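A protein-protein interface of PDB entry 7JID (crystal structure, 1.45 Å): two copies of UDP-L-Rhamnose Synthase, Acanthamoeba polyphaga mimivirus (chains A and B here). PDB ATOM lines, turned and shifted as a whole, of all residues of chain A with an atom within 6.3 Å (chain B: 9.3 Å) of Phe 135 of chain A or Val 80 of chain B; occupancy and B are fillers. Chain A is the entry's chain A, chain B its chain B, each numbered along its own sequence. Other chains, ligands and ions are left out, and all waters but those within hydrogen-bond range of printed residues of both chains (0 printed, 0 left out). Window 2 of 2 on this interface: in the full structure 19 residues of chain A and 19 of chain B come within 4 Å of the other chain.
The backbone NH of Tyr 88 of chain B is in hydrogen-bond range of the backbone carbonyl oxygen of Val 83 of chain B, 2.8 Å away. The backbone NH of Gly 89 of chain B is in hydrogen-bond range of the backbone carbonyl oxygen of Lys 84 of chain B.
Val 80 of chain B touches Phe 135 of chain A. OG of Ser 138 of chain A touches CD2 of Leu 79 of chain B, at 3.7 Å. Val 80 of chain B touches Val 141 of chain A. Val 80 of chain B touches Phe 145 of chain A. Phe 145 of chain A touches Val 83 of chain B (CD2 to CG1, 3.4 Å). Phe 145 of chain A touches Lys 84 of chain B. Phe 145 of chain A touches Tyr 88 of chain B.
Of the printed residues of chain B, Phe 135 of chain A touches Val 80. Val 80 of chain B touches three residues of chain A. Phe 134 of chain A touches none of the printed residues of chain B. No residue of chain B comes within 4 Å of Gly 136 of chain A. Of the printed residues of chain B, Ser 138 of chain A touches Leu 79. Printed residues of chain B within 4 Å of Phe 145 of chain A: Val 80 (3.9 Å), Val 83 (3.4 Å), Lys 84 (3.7 Å) and Tyr 88 (3.5 Å). Of the printed residues of chain B, Val 141 of chain A touches Val 80 (3.7 Å). Printed residues of chain A within 4 Å of Tyr 88 of chain B: Phe 145. Of the printed residues of chain A, Lys 84 of chain B touches Phe 145 (3.7 Å). The nearest printed residue of chain A that does not touch Lys 84 of chain B is Val 141 of chain A (6.7 Å).
Printed residues of chain A that touch a printed residue of chain B: Phe 135, Ser 138, Val 141 and Phe 145. Hydrophobic or aromatic side chains of chain A that line the printed part of chain B: Phe 135, Val 141 and Phe 145. Of the 21 printed residues of chain B, 5 touch a printed residue of chain A. Among the printed residues, no Asp or Glu carboxylate lies within 4 Å of a Lys or Arg side-chain nitrogen of the other chain.
Position printed for both chains: 138. Of the 7 pairs that touch across the chains among the printed residues, none has its exchanged pair printed and touching as well.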
ATOM      1  N   ILE A 112      -5.333  15.224  27.281  1.00  0.00           N
ATOM      2  CA  ILE A 112      -3.909  15.481  26.910  1.00  0.00           C
ATOM      3  C   ILE A 112      -3.287  14.180  26.428  1.00  0.00           C
ATOM      4  O   ILE A 112      -2.077  14.169  26.139  1.00  0.00           O
ATOM      5  CB  ILE A 112      -3.191  16.071  28.136  1.00  0.00           C
ATOM      6  CG1 ILE A 112      -3.155  15.089  29.304  1.00  0.00           C
ATOM      7  CG2 ILE A 112      -3.902  17.379  28.513  1.00  0.00           C
ATOM      8  CD1 ILE A 112      -2.461  15.600  30.531  1.00  0.00           C
ATOM      9  N   PRO A 132       1.911  14.140  28.208  1.00  0.00           N
ATOM     10  CA  PRO A 132       0.954  14.270  27.108  1.00  0.00           C
ATOM     11  C   PRO A 132       1.444  13.618  25.810  1.00  0.00           C
ATOM     12  O   PRO A 132       2.645  13.678  25.529  1.00  0.00           O
ATOM     13  CB  PRO A 132       0.854  15.786  26.929  1.00  0.00           C
ATOM     14  CG  PRO A 132       1.147  16.335  28.307  1.00  0.00           C
ATOM     15  CD  PRO A 132       2.251  15.432  28.829  1.00  0.00           C
ATOM     16  N   ASN A 133       0.530  12.992  25.091  1.00  0.00           N
ATOM     17  CA  ASN A 133       0.823  12.450  23.751  1.00  0.00           C
ATOM     18  C   ASN A 133      -0.275  12.820  22.777  1.00  0.00           C
ATOM     19  O   ASN A 133      -0.284  12.273  21.670  1.00  0.00           O
ATOM     20  CB  ASN A 133       1.062  10.945  23.793  1.00  0.00           C
ATOM     21  CG  ASN A 133      -0.221  10.152  23.836  1.00  0.00           C
ATOM     22  OD1 ASN A 133      -1.233  10.625  24.367  1.00  0.00           O
ATOM     23  ND2 ASN A 133      -0.207   8.993  23.210  1.00  0.00           N
ATOM     24  N   PHE A 134      -1.203  13.695  23.139  1.00  0.00           N
ATOM     25  CA  PHE A 134      -2.233  14.211  22.207  1.00  0.00           C
ATOM     26  C   PHE A 134      -2.033  15.713  21.989  1.00  0.00           C
ATOM     27  O   PHE A 134      -2.054  16.471  22.979  1.00  0.00           O
ATOM     28  CB  PHE A 134      -3.656  13.887  22.667  1.00  0.00           C
ATOM     29  CG  PHE A 134      -4.702  14.456  21.761  1.00  0.00           C
ATOM     30  CD1 PHE A 134      -4.943  13.933  20.488  1.00  0.00           C
ATOM     31  CD2 PHE A 134      -5.420  15.563  22.137  1.00  0.00           C
ATOM     32  CE1 PHE A 134      -5.875  14.524  19.652  1.00  0.00           C
ATOM     33  CE2 PHE A 134      -6.382  16.129  21.319  1.00  0.00           C
ATOM     34  CZ  PHE A 134      -6.624  15.603  20.076  1.00  0.00           C
ATOM     35  N   PHE A 135      -1.910  16.105  20.729  1.00  0.00           N
ATOM     36  CA  PHE A 135      -1.579  17.499  20.364  1.00  0.00           C
ATOM     37  C   PHE A 135      -2.543  18.016  19.308  1.00  0.00           C
ATOM     38  O   PHE A 135      -2.169  18.957  18.622  1.00  0.00           O
ATOM     39  CB  PHE A 135      -0.107  17.602  19.977  1.00  0.00           C
ATOM     40  CG  PHE A 135       0.828  16.959  20.953  1.00  0.00           C
ATOM     41  CD1 PHE A 135       1.119  17.573  22.167  1.00  0.00           C
ATOM     42  CD2 PHE A 135       1.503  15.779  20.643  1.00  0.00           C
ATOM     43  CE1 PHE A 135       1.998  16.991  23.071  1.00  0.00           C
ATOM     44  CE2 PHE A 135       2.385  15.199  21.565  1.00  0.00           C
ATOM     45  CZ  PHE A 135       2.641  15.814  22.773  1.00  0.00           C
ATOM     46  N   GLY A 136      -3.732  17.417  19.187  1.00  0.00           N
ATOM     47  CA  GLY A 136      -4.620  17.669  18.039  1.00  0.00           C
ATOM     48  C   GLY A 136      -5.602  18.802  18.210  1.00  0.00           C
ATOM     49  O   GLY A 136      -6.416  19.076  17.268  1.00  0.00           O
ATOM     50  N   SER A 137      -5.604  19.491  19.357  1.00  0.00           N
ATOM     51  CA  SER A 137      -6.367  20.749  19.526  1.00  0.00           C
ATOM     52  C   SER A 137      -5.419  21.734  20.232  1.00  0.00           C
ATOM     53  O   SER A 137      -4.553  21.307  21.038  1.00  0.00           O
ATOM     54  CB  SER A 137      -7.652  20.582  20.276  1.00  0.00           C
ATOM     55  OG  SER A 137      -7.391  20.211  21.626  1.00  0.00           O
ATOM     56  N   SER A 138      -5.624  23.021  20.043  1.00  0.00           N
ATOM     57  CA  SER A 138      -4.810  24.057  20.721  1.00  0.00           C
ATOM     58  C   SER A 138      -5.073  24.003  22.228  1.00  0.00           C
ATOM     59  O   SER A 138      -4.105  24.140  23.032  1.00  0.00           O
ATOM     60  CB  SER A 138      -5.049  25.411  20.126  1.00  0.00           C
ATOM     61  OG  SER A 138      -4.522  25.443  18.791  1.00  0.00           O
ATOM     62  N   SER A 140      -5.832  21.256  23.945  1.00  0.00           N
ATOM     63  CA  SER A 140      -5.176  20.061  24.503  1.00  0.00           C
ATOM     64  C   SER A 140      -3.676  20.330  24.614  1.00  0.00           C
ATOM     65  O   SER A 140      -3.020  19.927  25.599  1.00  0.00           O
ATOM     66  CB  SER A 140      -5.464  18.809  23.731  1.00  0.00           C
ATOM     67  OG  SER A 140      -6.797  18.379  23.963  1.00  0.00           O
ATOM     68  N   VAL A 141      -3.136  21.056  23.648  1.00  0.00           N
ATOM     69  CA  VAL A 141      -1.684  21.384  23.635  1.00  0.00           C
ATOM     70  C   VAL A 141      -1.339  22.239  24.855  1.00  0.00           C
ATOM     71  O   VAL A 141      -0.441  21.873  25.624  1.00  0.00           O
ATOM     72  CB  VAL A 141      -1.295  22.096  22.347  1.00  0.00           C
ATOM     73  CG1 VAL A 141       0.136  22.608  22.494  1.00  0.00           C
ATOM     74  CG2 VAL A 141      -1.406  21.129  21.172  1.00  0.00           C
ATOM     75  N   PHE A 145       0.728  21.219  28.643  1.00  0.00           N
ATOM     76  CA  PHE A 145       1.828  21.916  29.334  1.00  0.00           C
ATOM     77  C   PHE A 145       1.393  22.361  30.716  1.00  0.00           C
ATOM     78  O   PHE A 145       2.186  22.296  31.627  1.00  0.00           O
ATOM     79  CB  PHE A 145       2.369  23.063  28.484  1.00  0.00           C
ATOM     80  CG  PHE A 145       3.153  22.544  27.301  1.00  0.00           C
ATOM     81  CD1 PHE A 145       4.364  21.901  27.506  1.00  0.00           C
ATOM     82  CD2 PHE A 145       2.632  22.572  26.018  1.00  0.00           C
ATOM     83  CE1 PHE A 145       5.077  21.373  26.445  1.00  0.00           C
ATOM     84  CE2 PHE A 145       3.365  22.083  24.950  1.00  0.00           C
ATOM     85  CZ  PHE A 145       4.574  21.465  25.177  1.00  0.00           C
ATOM     86  N   ASP B  38      12.942  20.727  27.857  1.00  0.00           N
ATOM     87  CA  ASP B  38      11.539  20.260  28.064  1.00  0.00           C
ATOM     88  C   ASP B  38      11.514  18.858  28.676  1.00  0.00           C
ATOM     89  O   ASP B  38      10.436  18.371  29.019  1.00  0.00           O
ATOM     90  CB  ASP B  38      10.722  20.298  26.769  1.00  0.00           C
ATOM     91  CG  ASP B  38      11.356  19.511  25.637  1.00  0.00           C
ATOM     92  OD1 ASP B  38      12.355  20.005  25.130  1.00  0.00           O
ATOM     93  OD2 ASP B  38      10.810  18.431  25.256  1.00  0.00           O
ATOM     94  N   ARG B  61      12.233  28.378  19.585  1.00  0.00           N
ATOM     95  CA  ARG B  61      11.799  27.968  18.240  1.00  0.00           C
ATOM     96  C   ARG B  61      11.330  29.224  17.520  1.00  0.00           C
ATOM     97  O   ARG B  61      10.358  29.840  17.969  1.00  0.00           O
ATOM     98  CB  ARG B  61      10.718  26.885  18.347  1.00  0.00           C
ATOM     99  CG  ARG B  61      10.412  26.200  17.020  1.00  0.00           C
ATOM    100  CD  ARG B  61      11.565  25.320  16.509  1.00  0.00           C
ATOM    101  NE  ARG B  61      12.247  24.600  17.572  1.00  0.00           N
ATOM    102  CZ  ARG B  61      13.410  23.973  17.485  1.00  0.00           C
ATOM    103  NH1 ARG B  61      13.932  23.414  18.563  1.00  0.00           N
ATOM    104  NH2 ARG B  61      14.104  24.010  16.351  1.00  0.00           N
ATOM    105  N   TYR B  72       7.093  30.735  10.955  1.00  0.00           N
ATOM    106  CA  TYR B  72       7.096  29.255  11.067  1.00  0.00           C
ATOM    107  C   TYR B  72       6.064  28.800  12.107  1.00  0.00           C
ATOM    108  O   TYR B  72       5.385  27.787  11.913  1.00  0.00           O
ATOM    109  CB  TYR B  72       8.483  28.776  11.460  1.00  0.00           C
ATOM    110  CG  TYR B  72       8.584  27.329  11.862  1.00  0.00           C
ATOM    111  CD1 TYR B  72       8.617  26.323  10.914  1.00  0.00           C
ATOM    112  CD2 TYR B  72       8.667  26.964  13.194  1.00  0.00           C
ATOM    113  CE1 TYR B  72       8.714  24.992  11.278  1.00  0.00           C
ATOM    114  CE2 TYR B  72       8.788  25.640  13.573  1.00  0.00           C
ATOM    115  CZ  TYR B  72       8.820  24.649  12.608  1.00  0.00           C
ATOM    116  OH  TYR B  72       8.941  23.341  12.967  1.00  0.00           O
ATOM    117  N   LEU B  73       5.925  29.543  13.214  1.00  0.00           N
ATOM    118  CA  LEU B  73       5.088  29.068  14.349  1.00  0.00           C
ATOM    119  C   LEU B  73       3.608  29.305  14.073  1.00  0.00           C
ATOM    120  O   LEU B  73       2.772  28.811  14.900  1.00  0.00           O
ATOM    121  CB  LEU B  73       5.494  29.812  15.626  1.00  0.00           C
ATOM    122  CG  LEU B  73       6.953  29.648  16.046  1.00  0.00           C
ATOM    123  CD1 LEU B  73       7.276  30.622  17.164  1.00  0.00           C
ATOM    124  CD2 LEU B  73       7.215  28.221  16.482  1.00  0.00           C
ATOM    125  N   GLN B  75       1.918  28.108  11.437  1.00  0.00           N
ATOM    126  CA  GLN B  75       1.390  26.882  10.763  1.00  0.00           C
ATOM    127  C   GLN B  75       0.632  26.018  11.780  1.00  0.00           C
ATOM    128  O   GLN B  75       1.075  25.879  12.940  1.00  0.00           O
ATOM    129  CB  GLN B  75       2.516  26.046  10.160  1.00  0.00           C
ATOM    130  CG  GLN B  75       3.441  26.785   9.209  1.00  0.00           C
ATOM    131  CD  GLN B  75       4.553  25.876   8.751  1.00  0.00           C
ATOM    132  OE1 GLN B  75       4.400  25.118   7.792  1.00  0.00           O
ATOM    133  NE2 GLN B  75       5.668  25.900   9.477  1.00  0.00           N
ATOM    134  N   SER B  76      -0.481  25.425  11.368  1.00  0.00           N
ATOM    135  CA  SER B  76      -1.193  24.394  12.171  1.00  0.00           C
ATOM    136  C   SER B  76      -0.218  23.288  12.576  1.00  0.00           C
ATOM    137  O   SER B  76       0.565  22.817  11.711  1.00  0.00           O
ATOM    138  CB  SER B  76      -2.351  23.818  11.414  1.00  0.00           C
ATOM    139  OG  SER B  76      -3.351  24.793  11.270  1.00  0.00           O
ATOM    140  N   GLY B  77      -0.253  22.887  13.845  1.00  0.00           N
ATOM    141  CA  GLY B  77       0.602  21.819  14.376  1.00  0.00           C
ATOM    142  C   GLY B  77       1.893  22.347  14.960  1.00  0.00           C
ATOM    143  O   GLY B  77       2.657  21.544  15.533  1.00  0.00           O
ATOM    144  N   LYS B  78       2.172  23.652  14.854  1.00  0.00           N
ATOM    145  CA  LYS B  78       3.448  24.156  15.423  1.00  0.00           C
ATOM    146  C   LYS B  78       3.195  24.835  16.773  1.00  0.00           C
ATOM    147  O   LYS B  78       4.196  25.120  17.424  1.00  0.00           O
ATOM    148  CB  LYS B  78       4.221  25.087  14.488  1.00  0.00           C
ATOM    149  CG  LYS B  78       4.744  24.419  13.228  1.00  0.00           C
ATOM    150  CD  LYS B  78       5.658  23.245  13.477  1.00  0.00           C
ATOM    151  CE  LYS B  78       6.009  22.540  12.178  1.00  0.00           C
ATOM    152  NZ  LYS B  78       6.920  21.395  12.379  1.00  0.00           N
ATOM    153  N   LEU B  79       1.946  25.005  17.221  1.00  0.00           N
ATOM    154  CA  LEU B  79       1.794  25.543  18.602  1.00  0.00           C
ATOM    155  C   LEU B  79       2.577  24.675  19.590  1.00  0.00           C
ATOM    156  O   LEU B  79       3.158  25.213  20.575  1.00  0.00           O
ATOM    157  CB  LEU B  79       0.327  25.628  19.010  1.00  0.00           C
ATOM    158  CG  LEU B  79       0.095  26.176  20.418  1.00  0.00           C
ATOM    159  CD1 LEU B  79       0.651  27.594  20.536  1.00  0.00           C
ATOM    160  CD2 LEU B  79      -1.381  26.086  20.730  1.00  0.00           C
ATOM    161  N   VAL B  80       2.488  23.335  19.483  1.00  0.00           N
ATOM    162  CA  VAL B  80       3.203  22.442  20.443  1.00  0.00           C
ATOM    163  C   VAL B  80       4.710  22.771  20.483  1.00  0.00           C
ATOM    164  O   VAL B  80       5.295  22.757  21.608  1.00  0.00           O
ATOM    165  CB  VAL B  80       2.947  20.939  20.177  1.00  0.00           C
ATOM    166  CG1 VAL B  80       3.497  20.485  18.821  1.00  0.00           C
ATOM    167  CG2 VAL B  80       3.528  20.096  21.293  1.00  0.00           C
ATOM    168  N   GLU B  81       5.365  23.002  19.333  1.00  0.00           N
ATOM    169  CA  GLU B  81       6.809  23.364  19.306  1.00  0.00           C
ATOM    170  C   GLU B  81       7.016  24.735  19.979  1.00  0.00           C
ATOM    171  O   GLU B  81       7.950  24.911  20.717  1.00  0.00           O
ATOM    172  CB  GLU B  81       7.291  23.421  17.857  1.00  0.00           C
ATOM    173  CG  GLU B  81       7.141  22.111  17.134  1.00  0.00           C
ATOM    174  CD  GLU B  81       7.799  22.117  15.772  1.00  0.00           C
ATOM    175  OE1 GLU B  81       7.489  21.188  14.994  1.00  0.00           O
ATOM    176  OE2 GLU B  81       8.658  23.023  15.508  1.00  0.00           O
ATOM    177  N   ASN B  82       6.115  25.671  19.705  1.00  0.00           N
ATOM    178  CA  ASN B  82       6.134  27.037  20.256  1.00  0.00           C
ATOM    179  C   ASN B  82       6.131  26.947  21.785  1.00  0.00           C
ATOM    180  O   ASN B  82       7.083  27.434  22.430  1.00  0.00           O
ATOM    181  CB  ASN B  82       4.971  27.851  19.695  1.00  0.00           C
ATOM    182  CG  ASN B  82       5.032  29.331  20.031  1.00  0.00           C
ATOM    183  OD1 ASN B  82       5.966  29.786  20.716  1.00  0.00           O
ATOM    184  ND2 ASN B  82       4.042  30.066  19.531  1.00  0.00           N
ATOM    185  N   VAL B  83       5.097  26.328  22.357  1.00  0.00           N
ATOM    186  CA  VAL B  83       5.028  26.277  23.840  1.00  0.00           C
ATOM    187  C   VAL B  83       6.211  25.458  24.365  1.00  0.00           C
ATOM    188  O   VAL B  83       6.726  25.790  25.432  1.00  0.00           O
ATOM    189  CB  VAL B  83       3.672  25.753  24.336  1.00  0.00           C
ATOM    190  CG1 VAL B  83       3.606  25.813  25.844  1.00  0.00           C
ATOM    191  CG2 VAL B  83       2.538  26.567  23.730  1.00  0.00           C
ATOM    192  N   LYS B  84       6.528  24.315  23.750  1.00  0.00           N
ATOM    193  CA  LYS B  84       7.591  23.435  24.284  1.00  0.00           C
ATOM    194  C   LYS B  84       8.902  24.240  24.426  1.00  0.00           C
ATOM    195  O   LYS B  84       9.596  24.116  25.494  1.00  0.00           O
ATOM    196  CB  LYS B  84       7.811  22.265  23.324  1.00  0.00           C
ATOM    197  CG  LYS B  84       8.868  21.275  23.766  1.00  0.00           C
ATOM    198  CD  LYS B  84       9.394  20.456  22.592  1.00  0.00           C
ATOM    199  CE  LYS B  84       8.371  19.515  22.023  1.00  0.00           C
ATOM    200  NZ  LYS B  84       8.736  19.086  20.646  1.00  0.00           N
ATOM    201  N   ASP B  85       9.323  24.938  23.376  1.00  0.00           N
ATOM    202  CA  ASP B  85      10.699  25.488  23.264  1.00  0.00           C
ATOM    203  C   ASP B  85      10.741  26.929  23.773  1.00  0.00           C
ATOM    204  O   ASP B  85      11.796  27.356  24.255  1.00  0.00           O
ATOM    205  CB  ASP B  85      11.230  25.402  21.831  1.00  0.00           C
ATOM    206  CG  ASP B  85      11.364  23.979  21.291  1.00  0.00           C
ATOM    207  OD1 ASP B  85      11.484  23.041  22.099  1.00  0.00           O
ATOM    208  OD2 ASP B  85      11.279  23.837  20.051  1.00  0.00           O
ATOM    209  N   ASN B  86       9.616  27.654  23.657  1.00  0.00           N
ATOM    210  CA  ASN B  86       9.563  29.105  23.964  1.00  0.00           C
ATOM    211  C   ASN B  86       8.970  29.368  25.350  1.00  0.00           C
ATOM    212  O   ASN B  86       9.105  30.511  25.781  1.00  0.00           O
ATOM    213  CB  ASN B  86       8.795  29.881  22.903  1.00  0.00           C
ATOM    214  CG  ASN B  86       9.535  29.818  21.584  1.00  0.00           C
ATOM    215  OD1 ASN B  86      10.782  29.809  21.571  1.00  0.00           O
ATOM    216  ND2 ASN B  86       8.812  29.827  20.494  1.00  0.00           N
ATOM    217  N   LEU B  87       8.396  28.369  26.022  1.00  0.00           N
ATOM    218  CA  LEU B  87       7.861  28.544  27.382  1.00  0.00           C
ATOM    219  C   LEU B  87       8.228  27.366  28.298  1.00  0.00           C
ATOM    220  O   LEU B  87       8.796  27.591  29.395  1.00  0.00           O
ATOM    221  CB  LEU B  87       6.348  28.791  27.295  1.00  0.00           C
ATOM    222  CG  LEU B  87       5.674  29.156  28.614  1.00  0.00           C
ATOM    223  CD1 LEU B  87       4.432  29.961  28.250  1.00  0.00           C
ATOM    224  CD2 LEU B  87       5.303  27.918  29.436  1.00  0.00           C
ATOM    225  N   TYR B  88       7.808  26.153  27.963  1.00  0.00           N
ATOM    226  CA  TYR B  88       7.917  25.053  28.940  1.00  0.00           C
ATOM    227  C   TYR B  88       9.385  24.722  29.232  1.00  0.00           C
ATOM    228  O   TYR B  88       9.759  24.648  30.392  1.00  0.00           O
ATOM    229  CB  TYR B  88       7.187  23.801  28.454  1.00  0.00           C
ATOM    230  CG  TYR B  88       7.265  22.688  29.468  1.00  0.00           C
ATOM    231  CD1 TYR B  88       6.516  22.737  30.620  1.00  0.00           C
ATOM    232  CD2 TYR B  88       8.094  21.604  29.284  1.00  0.00           C
ATOM    233  CE1 TYR B  88       6.554  21.716  31.552  1.00  0.00           C
ATOM    234  CE2 TYR B  88       8.175  20.582  30.217  1.00  0.00           C
ATOM    235  CZ  TYR B  88       7.421  20.655  31.376  1.00  0.00           C
ATOM    236  OH  TYR B  88       7.487  19.699  32.355  1.00  0.00           O
ATOM    237  N   GLY B  89      10.204  24.564  28.213  1.00  0.00           N
ATOM    238  CA  GLY B  89      11.642  24.276  28.433  1.00  0.00           C
ATOM    239  C   GLY B  89      12.284  25.329  29.338  1.00  0.00           C
ATOM    240  O   GLY B  89      12.896  25.007  30.370  1.00  0.00           O
ATOM    241  N   SER B 138       2.256  34.607  17.226  1.00  0.00           N
ATOM    242  CA  SER B 138       2.145  33.470  18.156  1.00  0.00           C
ATOM    243  C   SER B 138       3.446  33.390  18.968  1.00  0.00           C
ATOM    244  O   SER B 138       3.357  33.211  20.190  1.00  0.00           O
ATOM    245  CB  SER B 138       1.830  32.207  17.383  1.00  0.00           C
ATOM    246  OG  SER B 138       0.464  32.260  16.978  1.00  0.00           O
ATOM    247  N   VAL B 142       3.389  33.771  23.168  1.00  0.00           N
ATOM    248  CA  VAL B 142       3.980  32.763  24.085  1.00  0.00           C
ATOM    249  C   VAL B 142       5.127  33.379  24.887  1.00  0.00           C
ATOM    250  O   VAL B 142       5.164  33.209  26.088  1.00  0.00           O
ATOM    251  CB  VAL B 142       4.398  31.526  23.284  1.00  0.00           C
ATOM    252  CG1 VAL B 142       5.287  30.609  24.113  1.00  0.00           C
ATOM    253  CG2 VAL B 142       3.151  30.799  22.841  1.00  0.00           C
